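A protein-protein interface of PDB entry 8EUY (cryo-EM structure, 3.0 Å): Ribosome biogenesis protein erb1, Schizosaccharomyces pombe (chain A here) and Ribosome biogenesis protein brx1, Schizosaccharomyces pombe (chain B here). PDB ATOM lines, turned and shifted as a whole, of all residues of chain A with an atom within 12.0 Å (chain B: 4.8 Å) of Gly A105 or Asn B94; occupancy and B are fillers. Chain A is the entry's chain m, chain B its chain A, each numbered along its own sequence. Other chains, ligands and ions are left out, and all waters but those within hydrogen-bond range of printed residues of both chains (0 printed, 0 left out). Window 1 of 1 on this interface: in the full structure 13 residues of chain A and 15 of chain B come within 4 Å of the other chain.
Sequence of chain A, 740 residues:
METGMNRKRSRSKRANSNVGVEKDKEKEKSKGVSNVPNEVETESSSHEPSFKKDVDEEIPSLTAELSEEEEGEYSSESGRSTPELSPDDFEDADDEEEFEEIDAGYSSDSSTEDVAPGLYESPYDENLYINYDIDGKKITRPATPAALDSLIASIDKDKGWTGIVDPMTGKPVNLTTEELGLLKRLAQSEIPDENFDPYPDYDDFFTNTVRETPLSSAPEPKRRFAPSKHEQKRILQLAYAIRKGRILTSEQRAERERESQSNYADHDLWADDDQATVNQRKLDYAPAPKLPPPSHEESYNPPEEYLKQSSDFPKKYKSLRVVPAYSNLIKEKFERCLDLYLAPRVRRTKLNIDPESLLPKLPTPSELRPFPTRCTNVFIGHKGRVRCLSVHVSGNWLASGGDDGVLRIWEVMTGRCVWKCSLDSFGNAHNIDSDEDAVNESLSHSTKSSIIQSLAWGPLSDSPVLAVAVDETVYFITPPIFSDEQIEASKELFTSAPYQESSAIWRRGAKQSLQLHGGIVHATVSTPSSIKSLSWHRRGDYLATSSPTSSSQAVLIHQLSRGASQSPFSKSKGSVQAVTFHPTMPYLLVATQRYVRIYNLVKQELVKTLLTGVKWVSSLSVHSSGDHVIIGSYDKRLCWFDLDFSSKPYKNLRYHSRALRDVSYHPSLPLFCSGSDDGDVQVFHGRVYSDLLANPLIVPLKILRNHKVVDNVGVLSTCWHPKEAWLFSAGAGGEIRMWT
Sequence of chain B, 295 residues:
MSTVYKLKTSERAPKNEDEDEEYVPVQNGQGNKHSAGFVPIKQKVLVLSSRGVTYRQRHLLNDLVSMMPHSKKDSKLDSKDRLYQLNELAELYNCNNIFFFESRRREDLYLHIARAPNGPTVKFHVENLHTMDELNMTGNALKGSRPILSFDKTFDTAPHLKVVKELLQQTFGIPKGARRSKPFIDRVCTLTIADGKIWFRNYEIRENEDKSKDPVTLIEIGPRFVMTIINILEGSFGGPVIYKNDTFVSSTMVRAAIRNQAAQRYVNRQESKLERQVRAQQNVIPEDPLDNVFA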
ATOM      1  N   GLU A 101       7.433   2.644 -16.323  1.00  0.00           N
ATOM      2  CA  GLU A 101       7.406   1.187 -16.383  1.00  0.00           C
ATOM      3  C   GLU A 101       6.235   0.633 -15.580  1.00  0.00           C
ATOM      4  O   GLU A 101       5.724   1.293 -14.676  1.00  0.00           O
ATOM      5  CB  GLU A 101       8.723   0.604 -15.867  1.00  0.00           C
ATOM      6  CG  GLU A 101       9.885   0.755 -16.833  1.00  0.00           C
ATOM      7  CD  GLU A 101      10.518   2.132 -16.773  1.00  0.00           C
ATOM      8  OE1 GLU A 101      10.133   2.928 -15.891  1.00  0.00           O
ATOM      9  OE2 GLU A 101      11.401   2.418 -17.608  1.00  0.00           O
ATOM     10  N   ILE A 102       5.810  -0.582 -15.917  1.00  0.00           N
ATOM     11  CA  ILE A 102       4.680  -1.220 -15.251  1.00  0.00           C
ATOM     12  C   ILE A 102       5.065  -2.492 -14.516  1.00  0.00           C
ATOM     13  O   ILE A 102       4.224  -3.041 -13.786  1.00  0.00           O
ATOM     14  CB  ILE A 102       3.535  -1.514 -16.243  1.00  0.00           C
ATOM     15  CG1 ILE A 102       3.966  -2.576 -17.254  1.00  0.00           C
ATOM     16  CG2 ILE A 102       3.109  -0.240 -16.957  1.00  0.00           C
ATOM     17  CD1 ILE A 102       2.809  -3.289 -17.907  1.00  0.00           C
ATOM     18  N   ASP A 103       6.288  -2.992 -14.690  1.00  0.00           N
ATOM     19  CA  ASP A 103       6.843  -4.165 -14.020  1.00  0.00           C
ATOM     20  C   ASP A 103       6.132  -5.461 -14.391  1.00  0.00           C
ATOM     21  O   ASP A 103       6.503  -6.518 -13.865  1.00  0.00           O
ATOM     22  CB  ASP A 103       6.836  -4.021 -12.490  1.00  0.00           C
ATOM     23  CG  ASP A 103       7.547  -2.769 -12.020  1.00  0.00           C
ATOM     24  OD1 ASP A 103       8.521  -2.351 -12.684  1.00  0.00           O
ATOM     25  OD2 ASP A 103       7.134  -2.200 -10.988  1.00  0.00           O
ATOM     26  N   ALA A 104       5.136  -5.421 -15.279  1.00  0.00           N
ATOM     27  CA  ALA A 104       4.411  -6.615 -15.718  1.00  0.00           C
ATOM     28  C   ALA A 104       3.869  -7.406 -14.533  1.00  0.00           C
ATOM     29  O   ALA A 104       3.944  -8.636 -14.489  1.00  0.00           O
ATOM     30  CB  ALA A 104       5.290  -7.498 -16.605  1.00  0.00           C
ATOM     31  N   GLY A 105       3.314  -6.692 -13.558  1.00  0.00           N
ATOM     32  CA  GLY A 105       2.803  -7.321 -12.356  1.00  0.00           C
ATOM     33  C   GLY A 105       1.546  -8.134 -12.578  1.00  0.00           C
ATOM     34  O   GLY A 105       1.243  -8.536 -13.705  1.00  0.00           O
ATOM     35  N   TYR A 106       0.805  -8.388 -11.503  1.00  0.00           N
ATOM     36  CA  TYR A 106      -0.423  -9.174 -11.594  1.00  0.00           C
ATOM     37  C   TYR A 106      -1.296  -8.840 -10.397  1.00  0.00           C
ATOM     38  O   TYR A 106      -0.921  -9.131  -9.257  1.00  0.00           O
ATOM     39  CB  TYR A 106      -0.107 -10.667 -11.643  1.00  0.00           C
ATOM     40  CG  TYR A 106      -1.103 -11.487 -12.427  1.00  0.00           C
ATOM     41  CD1 TYR A 106      -2.444 -11.510 -12.074  1.00  0.00           C
ATOM     42  CD2 TYR A 106      -0.700 -12.235 -13.523  1.00  0.00           C
ATOM     43  CE1 TYR A 106      -3.354 -12.261 -12.788  1.00  0.00           C
ATOM     44  CE2 TYR A 106      -1.603 -12.988 -14.244  1.00  0.00           C
ATOM     45  CZ  TYR A 106      -2.930 -12.997 -13.873  1.00  0.00           C
ATOM     46  OH  TYR A 106      -3.833 -13.745 -14.590  1.00  0.00           O
ATOM     47  N   SER A 107      -2.450  -8.231 -10.652  1.00  0.00           N
ATOM     48  CA  SER A 107      -3.357  -7.869  -9.577  1.00  0.00           C
ATOM     49  C   SER A 107      -4.030  -9.111  -9.000  1.00  0.00           C
ATOM     50  O   SER A 107      -4.125 -10.159  -9.644  1.00  0.00           O
ATOM     51  CB  SER A 107      -4.409  -6.878 -10.072  1.00  0.00           C
ATOM     52  OG  SER A 107      -3.913  -5.551 -10.045  1.00  0.00           O
ATOM     53  N   SER A 108      -4.501  -8.980  -7.761  1.00  0.00           N
ATOM     54  CA  SER A 108      -5.123 -10.085  -7.045  1.00  0.00           C
ATOM     55  C   SER A 108      -6.593 -10.270  -7.394  1.00  0.00           C
ATOM     56  O   SER A 108      -7.257 -11.108  -6.774  1.00  0.00           O
ATOM     57  CB  SER A 108      -4.979  -9.878  -5.536  1.00  0.00           C
ATOM     58  OG  SER A 108      -5.569  -8.655  -5.131  1.00  0.00           O
ATOM     59  N   ASP A 109      -7.119  -9.514  -8.359  1.00  0.00           N
ATOM     60  CA  ASP A 109      -8.536  -9.564  -8.695  1.00  0.00           C
ATOM     61  C   ASP A 109      -8.768  -9.804 -10.183  1.00  0.00           C
ATOM     62  O   ASP A 109      -9.874  -9.563 -10.676  1.00  0.00           O
ATOM     63  CB  ASP A 109      -9.229  -8.273  -8.257  1.00  0.00           C
ATOM     64  CG  ASP A 109      -8.351  -7.056  -8.450  1.00  0.00           C
ATOM     65  OD1 ASP A 109      -7.566  -7.036  -9.421  1.00  0.00           O
ATOM     66  OD2 ASP A 109      -8.430  -6.128  -7.623  1.00  0.00           O
ATOM     67  N   SER A 110      -7.753 -10.268 -10.905  1.00  0.00           N
ATOM     68  CA  SER A 110      -7.908 -10.529 -12.328  1.00  0.00           C
ATOM     69  C   SER A 110      -8.890 -11.672 -12.559  1.00  0.00           C
ATOM     70  O   SER A 110      -9.039 -12.571 -11.727  1.00  0.00           O
ATOM     71  CB  SER A 110      -6.558 -10.860 -12.962  1.00  0.00           C
ATOM     72  OG  SER A 110      -6.599 -10.691 -14.368  1.00  0.00           O
ATOM     73  N   SER A 111      -9.573 -11.621 -13.705  1.00  0.00           N
ATOM     74  CA  SER A 111     -10.566 -12.642 -14.022  1.00  0.00           C
ATOM     75  C   SER A 111      -9.927 -14.021 -14.115  1.00  0.00           C
ATOM     76  O   SER A 111     -10.491 -15.009 -13.631  1.00  0.00           O
ATOM     77  CB  SER A 111     -11.281 -12.288 -15.326  1.00  0.00           C
ATOM     78  OG  SER A 111     -12.350 -13.181 -15.579  1.00  0.00           O
ATOM     79  N   THR A 112      -8.753 -14.109 -14.736  1.00  0.00           N
ATOM     80  CA  THR A 112      -8.024 -15.367 -14.780  1.00  0.00           C
ATOM     81  C   THR A 112      -7.513 -15.732 -13.390  1.00  0.00           C
ATOM     82  O   THR A 112      -7.240 -14.864 -12.556  1.00  0.00           O
ATOM     83  CB  THR A 112      -6.856 -15.276 -15.761  1.00  0.00           C
ATOM     84  OG1 THR A 112      -5.941 -14.263 -15.323  1.00  0.00           O
ATOM     85  CG2 THR A 112      -7.359 -14.930 -17.154  1.00  0.00           C
ATOM     86  N   ALA B  36       1.037  -3.200  -5.727  1.00  0.00           N
ATOM     87  CA  ALA B  36       1.439  -2.941  -7.106  1.00  0.00           C
ATOM     88  C   ALA B  36       1.284  -4.186  -7.969  1.00  0.00           C
ATOM     89  O   ALA B  36       0.832  -4.104  -9.116  1.00  0.00           O
ATOM     90  CB  ALA B  36       2.881  -2.433  -7.147  1.00  0.00           C
ATOM     91  N   GLY B  37       1.654  -5.348  -7.436  1.00  0.00           N
ATOM     92  CA  GLY B  37       1.506  -6.593  -8.162  1.00  0.00           C
ATOM     93  C   GLY B  37       1.748  -7.816  -7.304  1.00  0.00           C
ATOM     94  O   GLY B  37       2.752  -7.894  -6.589  1.00  0.00           O
ATOM     95  N   PRO B  40       4.174 -11.468  -9.539  1.00  0.00           N
ATOM     96  CA  PRO B  40       4.347 -10.867 -10.869  1.00  0.00           C
ATOM     97  C   PRO B  40       5.046 -11.784 -11.861  1.00  0.00           C
ATOM     98  O   PRO B  40       6.247 -12.047 -11.746  1.00  0.00           O
ATOM     99  CB  PRO B  40       5.187  -9.617 -10.578  1.00  0.00           C
ATOM    100  CG  PRO B  40       5.950  -9.959  -9.347  1.00  0.00           C
ATOM    101  CD  PRO B  40       5.076 -10.876  -8.536  1.00  0.00           C
ATOM    102  N   LYS B  44       3.507 -10.564 -19.876  1.00  0.00           N
ATOM    103  CA  LYS B  44       2.063 -10.636 -20.042  1.00  0.00           C
ATOM    104  C   LYS B  44       1.695  -9.969 -21.358  1.00  0.00           C
ATOM    105  O   LYS B  44       2.342  -9.011 -21.786  1.00  0.00           O
ATOM    106  CB  LYS B  44       1.319  -9.975 -18.876  1.00  0.00           C
ATOM    107  CG  LYS B  44      -0.096 -10.496 -18.677  1.00  0.00           C
ATOM    108  CD  LYS B  44      -0.757  -9.859 -17.468  1.00  0.00           C
ATOM    109  CE  LYS B  44      -2.195 -10.324 -17.312  1.00  0.00           C
ATOM    110  NZ  LYS B  44      -2.898  -9.588 -16.225  1.00  0.00           N
ATOM    111  N   ALA B  90      -2.745  -1.236 -21.231  1.00  0.00           N
ATOM    112  CA  ALA B  90      -1.728  -2.171 -20.764  1.00  0.00           C
ATOM    113  C   ALA B  90      -1.379  -1.920 -19.303  1.00  0.00           C
ATOM    114  O   ALA B  90      -1.224  -2.868 -18.524  1.00  0.00           O
ATOM    115  CB  ALA B  90      -0.483  -2.068 -21.641  1.00  0.00           C
ATOM    116  N   GLU B  91      -1.251  -0.650 -18.914  1.00  0.00           N
ATOM    117  CA  GLU B  91      -0.956  -0.329 -17.522  1.00  0.00           C
ATOM    118  C   GLU B  91      -2.077  -0.788 -16.603  1.00  0.00           C
ATOM    119  O   GLU B  91      -1.822  -1.301 -15.507  1.00  0.00           O
ATOM    120  CB  GLU B  91      -0.718   1.174 -17.373  1.00  0.00           C
ATOM    121  CG  GLU B  91      -0.033   1.573 -16.079  1.00  0.00           C
ATOM    122  CD  GLU B  91      -1.003   1.712 -14.922  1.00  0.00           C
ATOM    123  OE1 GLU B  91      -2.180   2.048 -15.172  1.00  0.00           O
ATOM    124  OE2 GLU B  91      -0.591   1.482 -13.766  1.00  0.00           O
ATOM    125  N   LEU B  92      -3.328  -0.603 -17.028  1.00  0.00           N
ATOM    126  CA  LEU B  92      -4.461  -1.020 -16.208  1.00  0.00           C
ATOM    127  C   LEU B  92      -4.487  -2.532 -16.026  1.00  0.00           C
ATOM    128  O   LEU B  92      -4.748  -3.027 -14.925  1.00  0.00           O
ATOM    129  CB  LEU B  92      -5.764  -0.531 -16.838  1.00  0.00           C
ATOM    130  CG  LEU B  92      -7.047  -0.828 -16.067  1.00  0.00           C
ATOM    131  CD1 LEU B  92      -7.146   0.081 -14.859  1.00  0.00           C
ATOM    132  CD2 LEU B  92      -8.253  -0.657 -16.970  1.00  0.00           C
ATOM    133  N   TYR B  93      -4.219  -3.279 -17.093  1.00  0.00           N
ATOM    134  CA  TYR B  93      -4.274  -4.733 -17.050  1.00  0.00           C
ATOM    135  C   TYR B  93      -2.928  -5.366 -16.727  1.00  0.00           C
ATOM    136  O   TYR B  93      -2.828  -6.598 -16.716  1.00  0.00           O
ATOM    137  CB  TYR B  93      -4.798  -5.282 -18.381  1.00  0.00           C
ATOM    138  CG  TYR B  93      -6.294  -5.138 -18.555  1.00  0.00           C
ATOM    139  CD1 TYR B  93      -6.900  -3.890 -18.525  1.00  0.00           C
ATOM    140  CD2 TYR B  93      -7.100  -6.251 -18.740  1.00  0.00           C
ATOM    141  CE1 TYR B  93      -8.264  -3.754 -18.680  1.00  0.00           C
ATOM    142  CE2 TYR B  93      -8.465  -6.125 -18.895  1.00  0.00           C
ATOM    143  CZ  TYR B  93      -9.042  -4.874 -18.863  1.00  0.00           C
ATOM    144  OH  TYR B  93     -10.402  -4.742 -19.017  1.00  0.00           O
ATOM    145  N   ASN B  94      -1.901  -4.556 -16.465  1.00  0.00           N
ATOM    146  CA  ASN B  94      -0.579  -5.046 -16.071  1.00  0.00           C
ATOM    147  C   ASN B  94       0.005  -5.998 -17.112  1.00  0.00           C
ATOM    148  O   ASN B  94       0.595  -7.027 -16.779  1.00  0.00           O
ATOM    149  CB  ASN B  94      -0.626  -5.710 -14.694  1.00  0.00           C
ATOM    150  CG  ASN B  94      -0.285  -4.749 -13.576  1.00  0.00           C
ATOM    151  OD1 ASN B  94       0.597  -3.903 -13.717  1.00  0.00           O
ATOM    152  ND2 ASN B  94      -0.984  -4.874 -12.455  1.00  0.00           N
ATOM    153  N   CYS B  95      -0.162  -5.656 -18.386  1.00  0.00           N
ATOM    154  CA  CYS B  95       0.405  -6.416 -19.492  1.00  0.00           C
ATOM    155  C   CYS B  95       1.542  -5.611 -20.103  1.00  0.00           C
ATOM    156  O   CYS B  95       1.331  -4.482 -20.557  1.00  0.00           O
ATOM    157  CB  CYS B  95      -0.657  -6.732 -20.545  1.00  0.00           C
ATOM    158  SG  CYS B  95      -2.144  -7.528 -19.899  1.00  0.00           S
ATOM    159  N   ASN B  96       2.743  -6.187 -20.111  1.00  0.00           N
ATOM    160  CA  ASN B  96       3.902  -5.504 -20.671  1.00  0.00           C
ATOM    161  C   ASN B  96       3.975  -5.602 -22.187  1.00  0.00           C
ATOM    162  O   ASN B  96       4.747  -4.860 -22.802  1.00  0.00           O
ATOM    163  CB  ASN B  96       5.188  -6.062 -20.059  1.00  0.00           C
ATOM    164  CG  ASN B  96       5.241  -7.574 -20.099  1.00  0.00           C
ATOM    165  OD1 ASN B  96       4.284  -8.249 -19.720  1.00  0.00           O
ATOM    166  ND2 ASN B  96       6.361  -8.114 -20.558  1.00  0.00           N
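CG of Glu B91 touches CG2 of Ile A102, 3.7 Å away. Ile A102 touches Asn B94. Ile A102 touches Cys B95. CD1 of Ile A102 touches N of Asn B96, at 3.6 Å. Asn B94 touches Ala A104 (O to CA, 3.98 Å). Ala A104 touches Asn B96. Pro B40 touches Gly A105. Tyr A106 touches Gly B37 (O to C, 3.6 Å). Asn B94 touches Ser A107 (ND2 to OG, 3.9 Å).
The backbone carbonyl oxygen (O) of Gly A105 lies close to the backbone carbonyl oxygen (O) of Asn B94 (3.5 Å).
N of Lys B44 sits at hydrogen-bond distance from OD1 of Asn B96. The backbone carbonyl oxygen of Ala B90 is in hydrogen-bond range of the backbone NH of Cys B95, 3.0 Å away. The backbone carbonyl oxygen of Tyr B93 lies within hydrogen-bond range of the side-chain sulfur of Cys B95 (3.4 Å).
Of the printed residues of chain A, Asn B94 touches Ile A102, Ala A104, Gly A105 and Ser A107. No residue of chain A comes within 4 Å of Ala B36. Of chain A, only Gly A105 comes within 4 Å of Pro B40. Lys B44 touches none of the printed residues of chain A. No residue of chain A comes within 4 Å of Ala B90. Of chain A, only Ile A102 comes within 4 Å of Glu B91. No residue of chain A comes within 4 Å of Leu B92. Cys B95 touches just one residue of chain A: Ile A102 (3.3 Å). Asn B96 touches just these residues of chain A: Ile A102 and Ala A104. Printed residues of chain B within 4 Å of Tyr A106: Gly B37 (3.6 Å). Of the printed residues of chain B, Ser A107 touches Asn B94. Of the printed residues of chain B, Ile A102 touches Glu B91 (3.7 Å), Asn B94 (3.7 Å), Cys B95 (3.3 Å) and Asn B96 (3.6 Å). Printed residues of chain B within 4 Å of Ala A104: Asn B94 and Asn B96. Asp A103 touches none of the printed residues of chain B. Ser A111 touches none of the printed residues of chain B. The nearest printed residue of chain B that does not touch Gly A105 is Gly B37 (4.4 Å). The nearest printed residue of chain A that does not touch Asn B94 is Tyr A106 (4.1 Å).
Hydrophobic or aromatic side chains of chain B within 4 Å of the printed part of chain A: Pro B40. Printed residues of chain A that touch a printed residue of chain B: Ile A102, Ala A104, Gly A105, Tyr A106 and Ser A107. Hydrophobic or aromatic side chains of chain A within 4 Å of the printed part of chain B: Ile A102 and Ala A104. Among the printed residues, 10 pairs touch across the chains.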
